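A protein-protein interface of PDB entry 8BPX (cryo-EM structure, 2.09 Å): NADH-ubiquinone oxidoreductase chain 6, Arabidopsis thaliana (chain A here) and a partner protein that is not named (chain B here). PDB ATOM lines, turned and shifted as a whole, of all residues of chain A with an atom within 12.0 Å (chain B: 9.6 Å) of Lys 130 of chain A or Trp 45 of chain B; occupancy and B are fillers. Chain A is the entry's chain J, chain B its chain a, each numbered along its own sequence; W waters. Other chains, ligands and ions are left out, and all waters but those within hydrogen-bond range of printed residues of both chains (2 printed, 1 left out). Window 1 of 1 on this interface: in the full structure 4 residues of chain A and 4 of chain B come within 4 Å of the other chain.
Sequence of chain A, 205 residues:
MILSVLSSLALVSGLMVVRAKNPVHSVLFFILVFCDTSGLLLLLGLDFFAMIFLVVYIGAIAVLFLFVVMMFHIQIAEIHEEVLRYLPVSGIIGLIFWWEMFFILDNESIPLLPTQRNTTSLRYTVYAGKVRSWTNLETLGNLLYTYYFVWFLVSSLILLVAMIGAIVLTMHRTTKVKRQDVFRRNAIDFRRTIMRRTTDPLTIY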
ATOM      1  N   THR A 120      -1.392  19.538  21.883  1.00  0.00           N
ATOM      2  CA  THR A 120      -2.804  19.235  21.664  1.00  0.00           C
ATOM      3  C   THR A 120      -3.047  18.617  20.293  1.00  0.00           C
ATOM      4  O   THR A 120      -3.997  17.845  20.121  1.00  0.00           O
ATOM      5  CB  THR A 120      -3.648  20.498  21.827  1.00  0.00           C
ATOM      6  OG1 THR A 120      -3.314  21.436  20.796  1.00  0.00           O
ATOM      7  CG2 THR A 120      -3.400  21.135  23.187  1.00  0.00           C
ATOM      8  N   ARG A 123      -3.177  14.731  20.104  1.00  0.00           N
ATOM      9  CA  ARG A 123      -4.311  13.980  20.620  1.00  0.00           C
ATOM     10  C   ARG A 123      -4.980  13.225  19.477  1.00  0.00           C
ATOM     11  O   ARG A 123      -5.446  13.835  18.510  1.00  0.00           O
ATOM     12  CB  ARG A 123      -5.304  14.920  21.302  1.00  0.00           C
ATOM     13  CG  ARG A 123      -5.824  14.415  22.639  1.00  0.00           C
ATOM     14  CD  ARG A 123      -6.138  15.558  23.594  1.00  0.00           C
ATOM     15  NE  ARG A 123      -4.935  16.148  24.166  1.00  0.00           N
ATOM     16  CZ  ARG A 123      -4.923  17.221  24.945  1.00  0.00           C
ATOM     17  NH1 ARG A 123      -6.040  17.850  25.272  1.00  0.00           N
ATOM     18  NH2 ARG A 123      -3.762  17.674  25.409  1.00  0.00           N
ATOM     19  N   TYR A 124      -5.015  11.901  19.580  1.00  0.00           N
ATOM     20  CA  TYR A 124      -5.623  11.057  18.559  1.00  0.00           C
ATOM     21  C   TYR A 124      -7.073  10.772  18.930  1.00  0.00           C
ATOM     22  O   TYR A 124      -7.360  10.356  20.055  1.00  0.00           O
ATOM     23  CB  TYR A 124      -4.842   9.750  18.412  1.00  0.00           C
ATOM     24  CG  TYR A 124      -5.361   8.834  17.326  1.00  0.00           C
ATOM     25  CD1 TYR A 124      -5.570   9.303  16.034  1.00  0.00           C
ATOM     26  CD2 TYR A 124      -5.643   7.501  17.592  1.00  0.00           C
ATOM     27  CE1 TYR A 124      -6.042   8.475  15.043  1.00  0.00           C
ATOM     28  CE2 TYR A 124      -6.119   6.664  16.605  1.00  0.00           C
ATOM     29  CZ  TYR A 124      -6.317   7.156  15.333  1.00  0.00           C
ATOM     30  OH  TYR A 124      -6.790   6.325  14.352  1.00  0.00           O
ATOM     31  N   THR A 125      -7.981  10.992  17.983  1.00  0.00           N
ATOM     32  CA  THR A 125      -9.411  10.812  18.203  1.00  0.00           C
ATOM     33  C   THR A 125      -9.877   9.531  17.523  1.00  0.00           C
ATOM     34  O   THR A 125      -9.668   9.351  16.319  1.00  0.00           O
ATOM     35  CB  THR A 125     -10.202  12.008  17.673  1.00  0.00           C
ATOM     36  OG1 THR A 125      -9.921  13.158  18.480  1.00  0.00           O
ATOM     37  CG2 THR A 125     -11.691  11.722  17.701  1.00  0.00           C
ATOM     38  N   VAL A 126     -10.508   8.652  18.293  1.00  0.00           N
ATOM     39  CA  VAL A 126     -11.141   7.443  17.778  1.00  0.00           C
ATOM     40  C   VAL A 126     -12.644   7.669  17.832  1.00  0.00           C
ATOM     41  O   VAL A 126     -13.237   7.692  18.918  1.00  0.00           O
ATOM     42  CB  VAL A 126     -10.737   6.198  18.579  1.00  0.00           C
ATOM     43  CG1 VAL A 126     -11.343   4.944  17.956  1.00  0.00           C
ATOM     44  CG2 VAL A 126      -9.227   6.091  18.670  1.00  0.00           C
ATOM     45  N   TYR A 127     -13.269   7.835  16.666  1.00  0.00           N
ATOM     46  CA  TYR A 127     -14.698   8.112  16.640  1.00  0.00           C
ATOM     47  C   TYR A 127     -15.536   6.872  16.933  1.00  0.00           C
ATOM     48  O   TYR A 127     -16.727   7.006  17.229  1.00  0.00           O
ATOM     49  CB  TYR A 127     -15.109   8.699  15.287  1.00  0.00           C
ATOM     50  CG  TYR A 127     -14.524  10.052  14.954  1.00  0.00           C
ATOM     51  CD1 TYR A 127     -15.103  11.215  15.433  1.00  0.00           C
ATOM     52  CD2 TYR A 127     -13.413  10.167  14.124  1.00  0.00           C
ATOM     53  CE1 TYR A 127     -14.580  12.454  15.125  1.00  0.00           C
ATOM     54  CE2 TYR A 127     -12.883  11.402  13.807  1.00  0.00           C
ATOM     55  CZ  TYR A 127     -13.475  12.545  14.311  1.00  0.00           C
ATOM     56  OH  TYR A 127     -12.963  13.783  14.007  1.00  0.00           O
ATOM     57  N   ALA A 128     -14.942   5.677  16.867  1.00  0.00           N
ATOM     58  CA  ALA A 128     -15.717   4.451  17.042  1.00  0.00           C
ATOM     59  C   ALA A 128     -16.358   4.390  18.423  1.00  0.00           C
ATOM     60  O   ALA A 128     -17.523   3.996  18.560  1.00  0.00           O
ATOM     61  CB  ALA A 128     -14.832   3.230  16.805  1.00  0.00           C
ATOM     62  N   GLY A 129     -15.621   4.785  19.459  1.00  0.00           N
ATOM     63  CA  GLY A 129     -16.176   4.804  20.799  1.00  0.00           C
ATOM     64  C   GLY A 129     -17.159   5.926  21.061  1.00  0.00           C
ATOM     65  O   GLY A 129     -17.755   5.957  22.143  1.00  0.00           O
ATOM     66  N   LYS A 130     -17.351   6.832  20.104  1.00  0.00           N
ATOM     67  CA  LYS A 130     -18.219   7.990  20.274  1.00  0.00           C
ATOM     68  C   LYS A 130     -19.583   7.835  19.610  1.00  0.00           C
ATOM     69  O   LYS A 130     -20.404   8.752  19.701  1.00  0.00           O
ATOM     70  CB  LYS A 130     -17.533   9.247  19.728  1.00  0.00           C
ATOM     71  CG  LYS A 130     -16.493   9.854  20.645  1.00  0.00           C
ATOM     72  CD  LYS A 130     -15.641  10.873  19.912  1.00  0.00           C
ATOM     73  CE  LYS A 130     -14.342  11.138  20.644  1.00  0.00           C
ATOM     74  NZ  LYS A 130     -14.345  12.470  21.297  1.00  0.00           N
ATOM     75  N   VAL A 131     -19.836   6.713  18.931  1.00  0.00           N
ATOM     76  CA  VAL A 131     -21.125   6.517  18.271  1.00  0.00           C
ATOM     77  C   VAL A 131     -22.239   6.411  19.304  1.00  0.00           C
ATOM     78  O   VAL A 131     -23.303   7.019  19.157  1.00  0.00           O
ATOM     79  CB  VAL A 131     -21.070   5.272  17.363  1.00  0.00           C
ATOM     80  CG1 VAL A 131     -22.468   4.842  16.942  1.00  0.00           C
ATOM     81  CG2 VAL A 131     -20.175   5.518  16.148  1.00  0.00           C
ATOM     82  N   ARG A 132     -22.005   5.647  20.366  1.00  0.00           N
ATOM     83  CA  ARG A 132     -22.953   5.432  21.464  1.00  0.00           C
ATOM     84  C   ARG A 132     -22.192   5.553  22.776  1.00  0.00           C
ATOM     85  O   ARG A 132     -21.702   4.553  23.306  1.00  0.00           O
ATOM     86  CB  ARG A 132     -23.637   4.077  21.351  1.00  0.00           C
ATOM     87  CG  ARG A 132     -24.655   3.795  22.445  1.00  0.00           C
ATOM     88  CD  ARG A 132     -25.348   2.484  22.248  1.00  0.00           C
ATOM     89  NE  ARG A 132     -26.348   2.189  23.265  1.00  0.00           N
ATOM     90  CZ  ARG A 132     -27.211   1.188  23.191  1.00  0.00           C
ATOM     91  NH1 ARG A 132     -27.228   0.371  22.150  1.00  0.00           N
ATOM     92  NH2 ARG A 132     -28.068   0.994  24.190  1.00  0.00           N
ATOM     93  N   SER A 133     -22.126   6.768  23.309  1.00  0.00           N
ATOM     94  CA  SER A 133     -21.417   6.996  24.557  1.00  0.00           C
ATOM     95  C   SER A 133     -22.294   6.613  25.742  1.00  0.00           C
ATOM     96  O   SER A 133     -23.513   6.793  25.717  1.00  0.00           O
ATOM     97  CB  SER A 133     -20.983   8.459  24.671  1.00  0.00           C
ATOM     98  OG  SER A 133     -22.036   9.330  24.288  1.00  0.00           O
ATOM     99  N   TRP A 134     -21.662   6.063  26.772  1.00  0.00           N
ATOM    100  CA  TRP A 134     -22.342   5.661  27.994  1.00  0.00           C
ATOM    101  C   TRP A 134     -22.146   6.720  29.069  1.00  0.00           C
ATOM    102  O   TRP A 134     -21.041   7.235  29.250  1.00  0.00           O
ATOM    103  CB  TRP A 134     -21.813   4.319  28.504  1.00  0.00           C
ATOM    104  CG  TRP A 134     -22.419   3.120  27.849  1.00  0.00           C
ATOM    105  CD1 TRP A 134     -23.071   3.077  26.649  1.00  0.00           C
ATOM    106  CD2 TRP A 134     -22.430   1.779  28.359  1.00  0.00           C
ATOM    107  NE1 TRP A 134     -23.488   1.794  26.382  1.00  0.00           N
ATOM    108  CE2 TRP A 134     -23.107   0.979  27.417  1.00  0.00           C
ATOM    109  CE3 TRP A 134     -21.938   1.182  29.523  1.00  0.00           C
ATOM    110  CZ2 TRP A 134     -23.298  -0.390  27.601  1.00  0.00           C
ATOM    111  CZ3 TRP A 134     -22.129  -0.176  29.704  1.00  0.00           C
ATOM    112  CH2 TRP A 134     -22.801  -0.947  28.748  1.00  0.00           C
ATOM    113  N   THR A 135     -23.219   7.032  29.788  1.00  0.00           N
ATOM    114  CA  THR A 135     -23.078   7.861  30.974  1.00  0.00           C
ATOM    115  C   THR A 135     -22.377   7.081  32.087  1.00  0.00           C
ATOM    116  O   THR A 135     -22.327   5.848  32.084  1.00  0.00           O
ATOM    117  CB  THR A 135     -24.445   8.358  31.458  1.00  0.00           C
ATOM    118  OG1 THR A 135     -25.178   7.273  32.039  1.00  0.00           O
ATOM    119  CG2 THR A 135     -25.244   8.948  30.302  1.00  0.00           C
ATOM    120  N   GLU A 138     -25.004   4.686  33.618  1.00  0.00           N
ATOM    121  CA  GLU A 138     -25.301   3.410  32.982  1.00  0.00           C
ATOM    122  C   GLU A 138     -24.093   2.479  32.948  1.00  0.00           C
ATOM    123  O   GLU A 138     -24.266   1.258  33.017  1.00  0.00           O
ATOM    124  CB  GLU A 138     -25.891   3.635  31.588  1.00  0.00           C
ATOM    125  CG  GLU A 138     -25.032   4.355  30.587  1.00  0.00           C
ATOM    126  CD  GLU A 138     -25.870   5.233  29.662  1.00  0.00           C
ATOM    127  OE1 GLU A 138     -27.107   5.238  29.805  1.00  0.00           O
ATOM    128  OE2 GLU A 138     -25.297   5.917  28.795  1.00  0.00           O
ATOM    129  N   HIS B  39     -29.269  22.568  20.834  1.00  0.00           N
ATOM    130  CA  HIS B  39     -29.593  21.193  20.477  1.00  0.00           C
ATOM    131  C   HIS B  39     -29.600  20.336  21.739  1.00  0.00           C
ATOM    132  O   HIS B  39     -28.583  20.239  22.432  1.00  0.00           O
ATOM    133  CB  HIS B  39     -28.590  20.644  19.462  1.00  0.00           C
ATOM    134  CG  HIS B  39     -28.784  19.195  19.140  1.00  0.00           C
ATOM    135  ND1 HIS B  39     -27.748  18.285  19.155  1.00  0.00           N
ATOM    136  CD2 HIS B  39     -29.892  18.499  18.797  1.00  0.00           C
ATOM    137  CE1 HIS B  39     -28.210  17.091  18.834  1.00  0.00           C
ATOM    138  NE2 HIS B  39     -29.508  17.191  18.612  1.00  0.00           N
ATOM    139  N   GLY B  41     -29.339  17.152  23.905  1.00  0.00           N
ATOM    140  CA  GLY B  41     -28.635  15.894  23.785  1.00  0.00           C
ATOM    141  C   GLY B  41     -27.283  15.981  23.118  1.00  0.00           C
ATOM    142  O   GLY B  41     -26.888  15.042  22.418  1.00  0.00           O
ATOM    143  N   HIS B  42     -26.586  17.107  23.314  1.00  0.00           N
ATOM    144  CA  HIS B  42     -25.223  17.288  22.746  1.00  0.00           C
ATOM    145  C   HIS B  42     -24.269  16.300  23.422  1.00  0.00           C
ATOM    146  O   HIS B  42     -23.988  16.483  24.623  1.00  0.00           O
ATOM    147  CB  HIS B  42     -24.773  18.746  22.905  1.00  0.00           C
ATOM    148  CG  HIS B  42     -24.104  19.306  21.695  1.00  0.00           C
ATOM    149  ND1 HIS B  42     -24.815  19.759  20.601  1.00  0.00           N
ATOM    150  CD2 HIS B  42     -22.799  19.499  21.406  1.00  0.00           C
ATOM    151  CE1 HIS B  42     -23.976  20.202  19.686  1.00  0.00           C
ATOM    152  NE2 HIS B  42     -22.732  20.053  20.157  1.00  0.00           N
ATOM    153  N   ASP B  43     -23.793  15.299  22.680  1.00  0.00           N
ATOM    154  CA  ASP B  43     -22.929  14.272  23.240  1.00  0.00           C
ATOM    155  C   ASP B  43     -21.504  14.407  22.692  1.00  0.00           C
ATOM    156  O   ASP B  43     -21.169  15.376  22.001  1.00  0.00           O
ATOM    157  CB  ASP B  43     -23.522  12.882  22.978  1.00  0.00           C
ATOM    158  CG  ASP B  43     -23.706  12.576  21.497  1.00  0.00           C
ATOM    159  OD1 ASP B  43     -23.266  13.372  20.642  1.00  0.00           O
ATOM    160  OD2 ASP B  43     -24.294  11.521  21.189  1.00  0.00           O
ATOM    161  N   GLU B  44     -20.659  13.426  23.025  1.00  0.00           N
ATOM    162  CA  GLU B  44     -19.269  13.432  22.575  1.00  0.00           C
ATOM    163  C   GLU B  44     -19.174  13.536  21.058  1.00  0.00           C
ATOM    164  O   GLU B  44     -18.320  14.257  20.527  1.00  0.00           O
ATOM    165  CB  GLU B  44     -18.559  12.163  23.051  1.00  0.00           C
ATOM    166  CG  GLU B  44     -18.104  12.183  24.493  1.00  0.00           C
ATOM    167  CD  GLU B  44     -19.258  12.181  25.475  1.00  0.00           C
ATOM    168  OE1 GLU B  44     -20.315  11.595  25.165  1.00  0.00           O
ATOM    169  OE2 GLU B  44     -19.099  12.755  26.568  1.00  0.00           O
ATOM    170  N   TRP B  45     -20.044  12.816  20.349  1.00  0.00           N
ATOM    171  CA  TRP B  45     -20.024  12.833  18.892  1.00  0.00           C
ATOM    172  C   TRP B  45     -20.292  14.232  18.350  1.00  0.00           C
ATOM    173  O   TRP B  45     -19.603  14.694  17.435  1.00  0.00           O
ATOM    174  CB  TRP B  45     -21.049  11.838  18.345  1.00  0.00           C
ATOM    175  CG  TRP B  45     -21.108  11.795  16.850  1.00  0.00           C
ATOM    176  CD1 TRP B  45     -21.843  12.601  16.035  1.00  0.00           C
ATOM    177  CD2 TRP B  45     -20.399  10.895  15.991  1.00  0.00           C
ATOM    178  NE1 TRP B  45     -21.639  12.261  14.720  1.00  0.00           N
ATOM    179  CE2 TRP B  45     -20.756  11.215  14.666  1.00  0.00           C
ATOM    180  CE3 TRP B  45     -19.498   9.848  16.213  1.00  0.00           C
ATOM    181  CZ2 TRP B  45     -20.244  10.527  13.568  1.00  0.00           C
ATOM    182  CZ3 TRP B  45     -18.993   9.167  15.122  1.00  0.00           C
ATOM    183  CH2 TRP B  45     -19.365   9.510  13.816  1.00  0.00           C
ATOM    184  N   ASP B  46     -21.296  14.919  18.898  1.00  0.00           N
ATOM    185  CA  ASP B  46     -21.631  16.253  18.406  1.00  0.00           C
ATOM    186  C   ASP B  46     -20.504  17.244  18.673  1.00  0.00           C
ATOM    187  O   ASP B  46     -20.198  18.089  17.824  1.00  0.00           O
ATOM    188  CB  ASP B  46     -22.938  16.729  19.038  1.00  0.00           C
ATOM    189  CG  ASP B  46     -24.120  15.857  18.660  1.00  0.00           C
ATOM    190  OD1 ASP B  46     -24.253  15.511  17.470  1.00  0.00           O
ATOM    191  OD2 ASP B  46     -24.917  15.511  19.554  1.00  0.00           O
ATOM    192  N   VAL B  47     -19.876  17.152  19.848  1.00  0.00           N
ATOM    193  CA  VAL B  47     -18.759  18.035  20.177  1.00  0.00           C
ATOM    194  C   VAL B  47     -17.586  17.794  19.233  1.00  0.00           C
ATOM    195  O   VAL B  47     -16.963  18.743  18.736  1.00  0.00           O
ATOM    196  CB  VAL B  47     -18.359  17.848  21.654  1.00  0.00           C
ATOM    197  CG1 VAL B  47     -17.123  18.649  21.976  1.00  0.00           C
ATOM    198  CG2 VAL B  47     -19.503  18.261  22.568  1.00  0.00           C
ATOM    199  N   ALA B  48     -17.261  16.523  18.976  1.00  0.00           N
ATOM    200  CA  ALA B  48     -16.195  16.210  18.029  1.00  0.00           C
ATOM    201  C   ALA B  48     -16.538  16.703  16.627  1.00  0.00           C
ATOM    202  O   ALA B  48     -15.664  17.195  15.903  1.00  0.00           O
ATOM    203  CB  ALA B  48     -15.919  14.706  18.019  1.00  0.00           C
ATOM    204  N   MET B  49     -17.808  16.585  16.231  1.00  0.00           N
ATOM    205  CA  MET B  49     -18.244  17.091  14.934  1.00  0.00           C
ATOM    206  C   MET B  49     -18.042  18.595  14.827  1.00  0.00           C
ATOM    207  O   MET B  49     -17.541  19.089  13.815  1.00  0.00           O
ATOM    208  CB  MET B  49     -19.711  16.731  14.690  1.00  0.00           C
ATOM    209  CG  MET B  49     -20.051  15.278  14.296  1.00  0.00           C
ATOM    210  SD  MET B  49     -18.972  14.356  13.162  1.00  0.00           S
ATOM    211  CE  MET B  49     -17.555  13.925  14.166  1.00  0.00           C
ATOM    212  N   GLU B  50     -18.436  19.344  15.859  1.00  0.00           N
ATOM    213  CA  GLU B  50     -18.261  20.795  15.825  1.00  0.00           C
ATOM    214  C   GLU B  50     -16.785  21.185  15.793  1.00  0.00           C
ATOM    215  O   GLU B  50     -16.388  22.079  15.028  1.00  0.00           O
ATOM    216  CB  GLU B  50     -18.977  21.436  17.015  1.00  0.00           C
ATOM    217  CG  GLU B  50     -20.495  21.314  16.957  1.00  0.00           C
ATOM    218  CD  GLU B  50     -21.197  21.887  18.173  1.00  0.00           C
ATOM    219  OE1 GLU B  50     -20.499  22.214  19.159  1.00  0.00           O
ATOM    220  OE2 GLU B  50     -22.442  21.980  18.165  1.00  0.00           O
ATOM    221  N   ARG B  51     -15.953  20.520  16.599  1.00  0.00           N
ATOM    222  CA  ARG B  51     -14.530  20.848  16.598  1.00  0.00           C
ATOM    223  C   ARG B  51     -13.889  20.548  15.246  1.00  0.00           C
ATOM    224  O   ARG B  51     -13.083  21.342  14.750  1.00  0.00           O
ATOM    225  CB  ARG B  51     -13.803  20.100  17.717  1.00  0.00           C
ATOM    226  CG  ARG B  51     -13.941  20.755  19.082  1.00  0.00           C
ATOM    227  CD  ARG B  51     -13.932  19.723  20.194  1.00  0.00           C
ATOM    228  NE  ARG B  51     -14.395  20.272  21.461  1.00  0.00           N
ATOM    229  CZ  ARG B  51     -13.972  19.867  22.651  1.00  0.00           C
ATOM    230  NH1 ARG B  51     -13.051  18.926  22.774  1.00  0.00           N
ATOM    231  NH2 ARG B  51     -14.494  20.414  23.744  1.00  0.00           N
ATOM    232  N   ARG B  52     -14.231  19.412  14.633  1.00  0.00           N
ATOM    233  CA  ARG B  52     -13.677  19.098  13.319  1.00  0.00           C
ATOM    234  C   ARG B  52     -14.249  20.008  12.235  1.00  0.00           C
ATOM    235  O   ARG B  52     -13.546  20.351  11.273  1.00  0.00           O
ATOM    236  CB  ARG B  52     -13.928  17.625  12.999  1.00  0.00           C
ATOM    237  CG  ARG B  52     -13.567  17.200  11.597  1.00  0.00           C
ATOM    238  CD  ARG B  52     -14.643  16.310  11.018  1.00  0.00           C
ATOM    239  NE  ARG B  52     -14.470  16.077   9.591  1.00  0.00           N
ATOM    240  CZ  ARG B  52     -15.315  16.497   8.660  1.00  0.00           C
ATOM    241  NH1 ARG B  52     -16.396  17.193   8.969  1.00  0.00           N
ATOM    242  NH2 ARG B  52     -15.068  16.213   7.384  1.00  0.00           N
ATOM    243  N   ASP B  53     -15.506  20.435  12.389  1.00  0.00           N
ATOM    244  CA  ASP B  53     -16.130  21.302  11.399  1.00  0.00           C
ATOM    245  C   ASP B  53     -15.524  22.692  11.416  1.00  0.00           C
ATOM    246  O   ASP B  53     -15.478  23.352  10.374  1.00  0.00           O
ATOM    247  CB  ASP B  53     -17.638  21.381  11.639  1.00  0.00           C
ATOM    248  CG  ASP B  53     -18.415  20.428  10.757  1.00  0.00           C
ATOM    249  OD1 ASP B  53     -17.817  19.440  10.285  1.00  0.00           O
ATOM    250  OD2 ASP B  53     -19.621  20.661  10.538  1.00  0.00           O
HETATM  251  O   HOH W   1     -13.391  15.923  15.963  1.00  0.00           O
HETATM  252  O   HOH W   2     -21.630  10.334  21.739  1.00  0.00           O
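The indole nitrogen of Trp 45 of chain B lies close to the side-chain sulfur of Met 49 of chain B. The backbone NH (N) of Trp 45 of chain B lies close to the side-chain carboxylate (OD1) of Asp 43 of chain B, at 3.3 Å.
Val 126 of chain A touches none of the printed residues of chain B. Of the printed residues of chain B, Tyr 127 of chain A touches Trp 45 (3.8 Å), Ala 48 (3.9 Å) and Met 49 (3.5 Å). No residue of chain B comes within 4 Å of Ala 128 of chain A. Lys 130 of chain A touches just these residues of chain B: Glu 44 and Trp 45. Of chain B, only Trp 45 (3.97 Å) comes within 4 Å of Val 131 of chain A. Of the printed residues of chain B, Ser 133 of chain A touches Glu 44. No residue of chain A comes within 4 Å of Asp 43 of chain B. Of chain A, only Lys 130 and Ser 133 come within 4 Å of Glu 44 of chain B. Trp 45 of chain B touches just these residues of chain A: Tyr 127, Lys 130 and Val 131. No residue of chain A comes within 4 Å of Asp 46 of chain B. No residue of chain A comes within 4 Å of Val 47 of chain B. Ala 48 of chain B touches one residue of chain A. Met 49 of chain B touches just one residue of chain A: Tyr 127 (3.5 Å). The nearest residue of chain B that does not touch Lys 130 of chain A is Ala 48 of chain B (4.3 Å). The nearest printed residue of chain B that does not touch Tyr 127 of chain A is Arg 52 of chain B (4.1 Å).
Among the printed residues, pairs that only touch across the chains: Lys 130 of chain A with Trp 45 of chain B, Tyr 127 of chain A with Met 49 of chain B, Tyr 127 of chain A with Trp 45 of chain B, Tyr 127 of chain A with Ala 48 of chain B, Lys 130 of chain A with Glu 44 of chain B and Val 131 of chain A with Trp 45 of chain B.
The side-chain hydroxyl of Ser 133 of chain A is in hydrogen-bond range of the side-chain carboxylate of Glu 44 of chain B (3.0 Å).
Water W1 lies within hydrogen-bond range of the backbone carbonyl oxygen of Ala 48 of chain B and the side-chain hydroxyl of Tyr 127 of chain A. Water W2 lies within hydrogen-bond range of the side-chain hydroxyl of Ser 133 of chain A (2.8 Å), the backbone carbonyl oxygen of Lys 130 of chain A (2.9 Å), the side-chain carboxylate of Asp 43 of chain B (3.0 Å), the backbone NH of Trp 45 of chain B (3.3 Å) and the backbone NH of Glu 44 of chain B (3.5 Å).
Printed residues of chain B that touch a printed residue of chain A: Glu 44, Trp 45, Ala 48 and Met 49. Hydrophobic or aromatic side chains of chain A within 4 Å of the printed part of chain B: Tyr 127 and Val 131. Among the printed residues, no Asp or Glu carboxylate lies within 4 Å of a Lys or Arg side-chain nitrogen of the other chain.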
